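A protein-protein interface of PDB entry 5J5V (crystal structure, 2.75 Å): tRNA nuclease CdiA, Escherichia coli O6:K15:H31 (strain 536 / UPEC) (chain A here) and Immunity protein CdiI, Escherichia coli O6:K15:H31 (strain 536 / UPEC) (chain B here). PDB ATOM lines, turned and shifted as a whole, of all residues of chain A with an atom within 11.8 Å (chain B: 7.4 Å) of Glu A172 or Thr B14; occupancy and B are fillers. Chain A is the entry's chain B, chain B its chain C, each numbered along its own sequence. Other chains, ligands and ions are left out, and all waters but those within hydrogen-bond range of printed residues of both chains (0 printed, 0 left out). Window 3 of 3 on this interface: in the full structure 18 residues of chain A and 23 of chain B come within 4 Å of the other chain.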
ATOM      1  N   PRO A 168      36.900  17.002  -2.545  1.00  0.00           N
ATOM      2  CA  PRO A 168      36.095  15.789  -2.520  1.00  0.00           C
ATOM      3  C   PRO A 168      34.954  15.944  -1.528  1.00  0.00           C
ATOM      4  O   PRO A 168      34.952  16.837  -0.685  1.00  0.00           O
ATOM      5  CB  PRO A 168      37.087  14.720  -2.074  1.00  0.00           C
ATOM      6  CG  PRO A 168      38.037  15.441  -1.263  1.00  0.00           C
ATOM      7  CD  PRO A 168      38.145  16.822  -1.784  1.00  0.00           C
ATOM      8  N   VAL A 169      33.945  15.090  -1.687  1.00  0.00           N
ATOM      9  CA  VAL A 169      32.751  15.157  -0.853  1.00  0.00           C
ATOM     10  C   VAL A 169      33.043  14.563   0.510  1.00  0.00           C
ATOM     11  O   VAL A 169      33.324  13.367   0.607  1.00  0.00           O
ATOM     12  CB  VAL A 169      31.571  14.420  -1.486  1.00  0.00           C
ATOM     13  CG1 VAL A 169      30.379  14.537  -0.584  1.00  0.00           C
ATOM     14  CG2 VAL A 169      31.268  14.978  -2.843  1.00  0.00           C
ATOM     15  N   PRO A 170      32.933  15.324   1.584  1.00  0.00           N
ATOM     16  CA  PRO A 170      33.274  14.770   2.897  1.00  0.00           C
ATOM     17  C   PRO A 170      32.214  13.806   3.401  1.00  0.00           C
ATOM     18  O   PRO A 170      31.019  13.990   3.187  1.00  0.00           O
ATOM     19  CB  PRO A 170      33.370  16.009   3.793  1.00  0.00           C
ATOM     20  CG  PRO A 170      32.607  17.058   3.085  1.00  0.00           C
ATOM     21  CD  PRO A 170      32.719  16.780   1.624  1.00  0.00           C
ATOM     22  N   LYS A 171      32.674  12.765   4.070  1.00  0.00           N
ATOM     23  CA  LYS A 171      31.815  11.924   4.880  1.00  0.00           C
ATOM     24  C   LYS A 171      31.730  12.476   6.301  1.00  0.00           C
ATOM     25  O   LYS A 171      32.488  13.361   6.694  1.00  0.00           O
ATOM     26  CB  LYS A 171      32.330  10.489   4.919  1.00  0.00           C
ATOM     27  CG  LYS A 171      32.534   9.791   3.603  1.00  0.00           C
ATOM     28  CD  LYS A 171      33.317   8.529   3.850  1.00  0.00           C
ATOM     29  CE  LYS A 171      33.523   7.709   2.612  1.00  0.00           C
ATOM     30  NZ  LYS A 171      34.250   6.458   2.916  1.00  0.00           N
ATOM     31  N   GLU A 172      30.811  11.914   7.087  1.00  0.00           N
ATOM     32  CA  GLU A 172      30.665  12.319   8.482  1.00  0.00           C
ATOM     33  C   GLU A 172      31.635  11.588   9.410  1.00  0.00           C
ATOM     34  O   GLU A 172      32.073  12.162  10.411  1.00  0.00           O
ATOM     35  CB  GLU A 172      29.231  12.055   8.937  1.00  0.00           C
ATOM     36  CG  GLU A 172      28.529  13.212   9.601  1.00  0.00           C
ATOM     37  CD  GLU A 172      27.085  12.880   9.961  1.00  0.00           C
ATOM     38  OE1 GLU A 172      26.841  11.789  10.529  1.00  0.00           O
ATOM     39  OE2 GLU A 172      26.195  13.705   9.672  1.00  0.00           O
ATOM     40  N   ASN A 173      31.971  10.329   9.107  1.00  0.00           N
ATOM     41  CA  ASN A 173      33.036   9.609   9.808  1.00  0.00           C
ATOM     42  C   ASN A 173      34.388  10.311   9.782  1.00  0.00           C
ATOM     43  O   ASN A 173      35.259   9.978  10.593  1.00  0.00           O
ATOM     44  CB  ASN A 173      33.209   8.197   9.235  1.00  0.00           C
ATOM     45  CG  ASN A 173      33.920   8.194   7.911  1.00  0.00           C
ATOM     46  OD1 ASN A 173      33.382   8.681   6.936  1.00  0.00           O
ATOM     47  ND2 ASN A 173      35.162   7.736   7.887  1.00  0.00           N
ATOM     48  N   GLY A 174      34.607  11.241   8.860  1.00  0.00           N
ATOM     49  CA  GLY A 174      35.958  11.664   8.566  1.00  0.00           C
ATOM     50  C   GLY A 174      36.506  10.916   7.368  1.00  0.00           C
ATOM     51  O   GLY A 174      36.328   9.701   7.239  1.00  0.00           O
ATOM     52  N   GLY A 175      37.170  11.629   6.476  1.00  0.00           N
ATOM     53  CA  GLY A 175      37.489  11.080   5.178  1.00  0.00           C
ATOM     54  C   GLY A 175      36.473  11.528   4.152  1.00  0.00           C
ATOM     55  O   GLY A 175      35.576  12.330   4.418  1.00  0.00           O
ATOM     56  N   TYR A 176      36.632  11.013   2.942  1.00  0.00           N
ATOM     57  CA  TYR A 176      35.905  11.570   1.820  1.00  0.00           C
ATOM     58  C   TYR A 176      35.393  10.451   0.925  1.00  0.00           C
ATOM     59  O   TYR A 176      35.928   9.343   0.919  1.00  0.00           O
ATOM     60  CB  TYR A 176      36.797  12.549   1.048  1.00  0.00           C
ATOM     61  CG  TYR A 176      37.325  13.685   1.906  1.00  0.00           C
ATOM     62  CD1 TYR A 176      38.477  13.540   2.659  1.00  0.00           C
ATOM     63  CD2 TYR A 176      36.661  14.901   1.969  1.00  0.00           C
ATOM     64  CE1 TYR A 176      38.953  14.567   3.448  1.00  0.00           C
ATOM     65  CE2 TYR A 176      37.131  15.939   2.751  1.00  0.00           C
ATOM     66  CZ  TYR A 176      38.280  15.765   3.493  1.00  0.00           C
ATOM     67  OH  TYR A 176      38.758  16.793   4.282  1.00  0.00           O
ATOM     68  N   TRP A 177      34.321  10.742   0.197  1.00  0.00           N
ATOM     69  CA  TRP A 177      34.010   9.947  -0.979  1.00  0.00           C
ATOM     70  C   TRP A 177      34.979  10.294  -2.096  1.00  0.00           C
ATOM     71  O   TRP A 177      35.413  11.437  -2.232  1.00  0.00           O
ATOM     72  CB  TRP A 177      32.580  10.192  -1.447  1.00  0.00           C
ATOM     73  CG  TRP A 177      31.532   9.863  -0.451  1.00  0.00           C
ATOM     74  CD1 TRP A 177      30.817  10.739   0.302  1.00  0.00           C
ATOM     75  CD2 TRP A 177      31.053   8.565  -0.114  1.00  0.00           C
ATOM     76  NE1 TRP A 177      29.935  10.067   1.098  1.00  0.00           N
ATOM     77  CE2 TRP A 177      30.060   8.727   0.856  1.00  0.00           C
ATOM     78  CE3 TRP A 177      31.374   7.282  -0.532  1.00  0.00           C
ATOM     79  CZ2 TRP A 177      29.385   7.660   1.404  1.00  0.00           C
ATOM     80  CZ3 TRP A 177      30.708   6.230   0.017  1.00  0.00           C
ATOM     81  CH2 TRP A 177      29.730   6.420   0.977  1.00  0.00           C
ATOM     82  N   ASP A 178      35.298   9.299  -2.911  1.00  0.00           N
ATOM     83  CA  ASP A 178      36.294   9.427  -3.969  1.00  0.00           C
ATOM     84  C   ASP A 178      35.606   9.170  -5.305  1.00  0.00           C
ATOM     85  O   ASP A 178      35.488   8.029  -5.751  1.00  0.00           O
ATOM     86  CB  ASP A 178      37.448   8.458  -3.734  1.00  0.00           C
ATOM     87  CG  ASP A 178      38.676   8.799  -4.540  1.00  0.00           C
ATOM     88  OD1 ASP A 178      38.539   9.339  -5.658  1.00  0.00           O
ATOM     89  OD2 ASP A 178      39.786   8.481  -4.068  1.00  0.00           O
ATOM     90  N   GLY B   9      26.422   2.877  10.554  1.00  0.00           N
ATOM     91  CA  GLY B   9      25.429   3.927  10.562  1.00  0.00           C
ATOM     92  C   GLY B   9      25.474   4.666   9.235  1.00  0.00           C
ATOM     93  O   GLY B   9      26.062   4.207   8.258  1.00  0.00           O
ATOM     94  N   ASN B  10      24.823   5.826   9.203  1.00  0.00           N
ATOM     95  CA  ASN B  10      24.804   6.630   7.990  1.00  0.00           C
ATOM     96  C   ASN B  10      25.923   7.664   8.098  1.00  0.00           C
ATOM     97  O   ASN B  10      25.826   8.640   8.852  1.00  0.00           O
ATOM     98  CB  ASN B  10      23.436   7.265   7.771  1.00  0.00           C
ATOM     99  CG  ASN B  10      23.348   8.035   6.479  1.00  0.00           C
ATOM    100  OD1 ASN B  10      24.359   8.365   5.871  1.00  0.00           O
ATOM    101  ND2 ASN B  10      22.123   8.260   6.009  1.00  0.00           N
ATOM    102  N   ILE B  11      26.992   7.429   7.333  1.00  0.00           N
ATOM    103  CA  ILE B  11      28.167   8.289   7.327  1.00  0.00           C
ATOM    104  C   ILE B  11      28.036   9.437   6.348  1.00  0.00           C
ATOM    105  O   ILE B  11      29.001  10.184   6.151  1.00  0.00           O
ATOM    106  CB  ILE B  11      29.420   7.478   6.961  1.00  0.00           C
ATOM    107  CG1 ILE B  11      29.257   6.946   5.545  1.00  0.00           C
ATOM    108  CG2 ILE B  11      29.620   6.347   7.926  1.00  0.00           C
ATOM    109  CD1 ILE B  11      30.407   6.158   5.055  1.00  0.00           C
ATOM    110  N   ASN B  12      26.882   9.584   5.707  1.00  0.00           N
ATOM    111  CA  ASN B  12      26.643  10.724   4.841  1.00  0.00           C
ATOM    112  C   ASN B  12      26.500  11.997   5.656  1.00  0.00           C
ATOM    113  O   ASN B  12      25.844  12.013   6.700  1.00  0.00           O
ATOM    114  CB  ASN B  12      25.381  10.501   4.009  1.00  0.00           C
ATOM    115  CG  ASN B  12      25.645   9.764   2.718  1.00  0.00           C
ATOM    116  OD1 ASN B  12      26.782   9.448   2.385  1.00  0.00           O
ATOM    117  ND2 ASN B  12      24.581   9.455   1.998  1.00  0.00           N
ATOM    118  N   MET B  13      27.126  13.067   5.177  1.00  0.00           N
ATOM    119  CA  MET B  13      26.742  14.400   5.597  1.00  0.00           C
ATOM    120  C   MET B  13      25.241  14.463   5.383  1.00  0.00           C
ATOM    121  O   MET B  13      24.741  14.103   4.309  1.00  0.00           O
ATOM    122  CB  MET B  13      27.460  15.490   4.796  1.00  0.00           C
ATOM    123  CG  MET B  13      28.912  15.746   5.191  1.00  0.00           C
ATOM    124  SD  MET B  13      29.178  16.182   7.089  1.00  0.00           S
ATOM    125  CE  MET B  13      31.044  16.771   7.042  1.00  0.00           C
ATOM    126  N   THR B  14      24.517  14.861   6.422  1.00  0.00           N
ATOM    127  CA  THR B  14      23.066  14.941   6.331  1.00  0.00           C
ATOM    128  C   THR B  14      22.678  16.068   5.379  1.00  0.00           C
ATOM    129  O   THR B  14      23.041  17.229   5.595  1.00  0.00           O
ATOM    130  CB  THR B  14      22.448  15.151   7.711  1.00  0.00           C
ATOM    131  OG1 THR B  14      22.535  13.929   8.450  1.00  0.00           O
ATOM    132  CG2 THR B  14      20.982  15.533   7.575  1.00  0.00           C
ATOM    133  N   LYS B  15      21.976  15.717   4.304  1.00  0.00           N
ATOM    134  CA  LYS B  15      21.432  16.713   3.394  1.00  0.00           C
ATOM    135  C   LYS B  15      20.352  16.056   2.550  1.00  0.00           C
ATOM    136  O   LYS B  15      20.268  14.834   2.462  1.00  0.00           O
ATOM    137  CB  LYS B  15      22.512  17.325   2.496  1.00  0.00           C
ATOM    138  CG  LYS B  15      23.538  16.355   1.953  1.00  0.00           C
ATOM    139  CD  LYS B  15      24.427  17.055   0.964  1.00  0.00           C
ATOM    140  CE  LYS B  15      25.869  16.630   1.093  1.00  0.00           C
ATOM    141  NZ  LYS B  15      26.667  16.976  -0.132  1.00  0.00           N
ATOM    142  N   GLU B  16      19.537  16.888   1.911  1.00  0.00           N
ATOM    143  CA  GLU B  16      18.441  16.351   1.135  1.00  0.00           C
ATOM    144  C   GLU B  16      18.954  15.760  -0.165  1.00  0.00           C
ATOM    145  O   GLU B  16      19.969  16.204  -0.690  1.00  0.00           O
ATOM    146  CB  GLU B  16      17.391  17.419   0.856  1.00  0.00           C
ATOM    147  CG  GLU B  16      16.650  17.818   2.133  1.00  0.00           C
ATOM    148  CD  GLU B  16      15.439  16.932   2.367  1.00  0.00           C
ATOM    149  OE1 GLU B  16      15.008  16.287   1.406  1.00  0.00           O
ATOM    150  OE2 GLU B  16      14.946  16.825   3.512  1.00  0.00           O
ATOM    151  N   GLN B  20      22.841  15.745  -3.073  1.00  0.00           N
ATOM    152  CA  GLN B  20      23.749  14.644  -2.798  1.00  0.00           C
ATOM    153  C   GLN B  20      24.483  14.230  -4.054  1.00  0.00           C
ATOM    154  O   GLN B  20      23.922  14.267  -5.146  1.00  0.00           O
ATOM    155  CB  GLN B  20      22.998  13.453  -2.216  1.00  0.00           C
ATOM    156  CG  GLN B  20      22.573  13.644  -0.791  1.00  0.00           C
ATOM    157  CD  GLN B  20      22.153  12.361  -0.137  1.00  0.00           C
ATOM    158  OE1 GLN B  20      21.248  11.694  -0.610  1.00  0.00           O
ATOM    159  NE2 GLN B  20      22.786  12.018   0.966  1.00  0.00           N
ATOM    160  N   GLU B  24      27.136   9.587  -2.482  1.00  0.00           N
ATOM    161  CA  GLU B  24      26.204   9.775  -1.378  1.00  0.00           C
ATOM    162  C   GLU B  24      24.850   9.160  -1.689  1.00  0.00           C
ATOM    163  O   GLU B  24      24.242   8.511  -0.834  1.00  0.00           O
ATOM    164  CB  GLU B  24      26.047  11.262  -1.079  1.00  0.00           C
ATOM    165  CG  GLU B  24      27.186  11.871  -0.314  1.00  0.00           C
ATOM    166  CD  GLU B  24      27.070  13.370  -0.183  1.00  0.00           C
ATOM    167  OE1 GLU B  24      26.884  14.050  -1.201  1.00  0.00           O
ATOM    168  OE2 GLU B  24      27.139  13.869   0.950  1.00  0.00           O
ATOM    169  N   GLU B  28      23.092   5.561   0.099  1.00  0.00           N
ATOM    170  CA  GLU B  28      21.758   5.465   0.672  1.00  0.00           C
ATOM    171  C   GLU B  28      20.915   4.374   0.013  1.00  0.00           C
ATOM    172  O   GLU B  28      19.928   3.935   0.605  1.00  0.00           O
ATOM    173  CB  GLU B  28      21.045   6.810   0.565  1.00  0.00           C
ATOM    174  CG  GLU B  28      21.803   7.979   1.127  1.00  0.00           C
ATOM    175  CD  GLU B  28      21.292   8.406   2.469  1.00  0.00           C
ATOM    176  OE1 GLU B  28      20.483   7.661   3.038  1.00  0.00           O
ATOM    177  OE2 GLU B  28      21.701   9.475   2.966  1.00  0.00           O
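O of Ile B11 is in hydrogen-bond range of N of Glu A172. OD1 of Asn B12 sits close to NE1 of Trp A177. O of Asn B12 sits close to OE2 of Glu A172.
The backbone carbonyl oxygen of Val A169 is in hydrogen-bond range of the backbone NH of Trp A177 (2.8 Å). The backbone NH (N) of Asn B12 sits at hydrogen-bond distance from the side-chain amide oxygen (OD1) of Asn B10, at 2.8 Å. ND2 of Asn B10 sits at hydrogen-bond distance from OE2 of Glu B28 (3.3 Å). O of Glu B24 is in hydrogen-bond range of ND2 of Asn B12 (3.0 Å). The side-chain amide nitrogen (ND2) of Asn B12 sits at hydrogen-bond distance from the side-chain carboxylate (OE2) of Glu B28, 3.0 Å away. The side-chain carboxylate of Glu B24 is in salt-bridge range of the side-chain amino group of Lys B15 (3.1 Å).
Glu B24 touches Val A169 (CD to CG1, 3.5 Å). Met B13 touches Pro A170 (CG to O, 3.4 Å). Ile B11 touches Lys A171. Lys A171 touches Met B13 (O to CE, 3.7 Å). Asn B10 touches Glu A172 (O to OE1, 3.7 Å). Glu A172 touches Met B13 (CG to SD, 3.9 Å). Glu A172 touches Thr B14 (OE2 to N, 3.8 Å). Trp A177 touches Glu B24 (NE1 to CG, 3.6 Å).
Printed residues of chain B within 4 Å of Pro A170: Met B13. Of chain B, only Asn B10 (3.7 Å), Ile B11 (2.7 Å), Asn B12 (3.4 Å), Met B13 (3.9 Å) and Thr B14 (3.8 Å) come within 4 Å of Glu A172. Of chain A, only Glu A172 (3.7 Å) comes within 4 Å of Asn B10. Of chain A, only Lys A171 and Glu A172 come within 4 Å of Ile B11. Of chain A, only Glu A172 and Trp A177 come within 4 Å of Asn B12. Thr B14 touches just one residue of chain A: Glu A172. Printed residues of chain A within 4 Å of Glu B24: Val A169 (3.5 Å) and Trp A177 (3.6 Å). The nearest residue of chain B that does not touch Glu A172 is Lys B15 (7.1 Å).
Hydrophobic or aromatic side chains of chain A within 4 Å of the printed part of chain B: Val A169 and Trp A177. Among the printed residues, 11 pairs touch across the chains.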
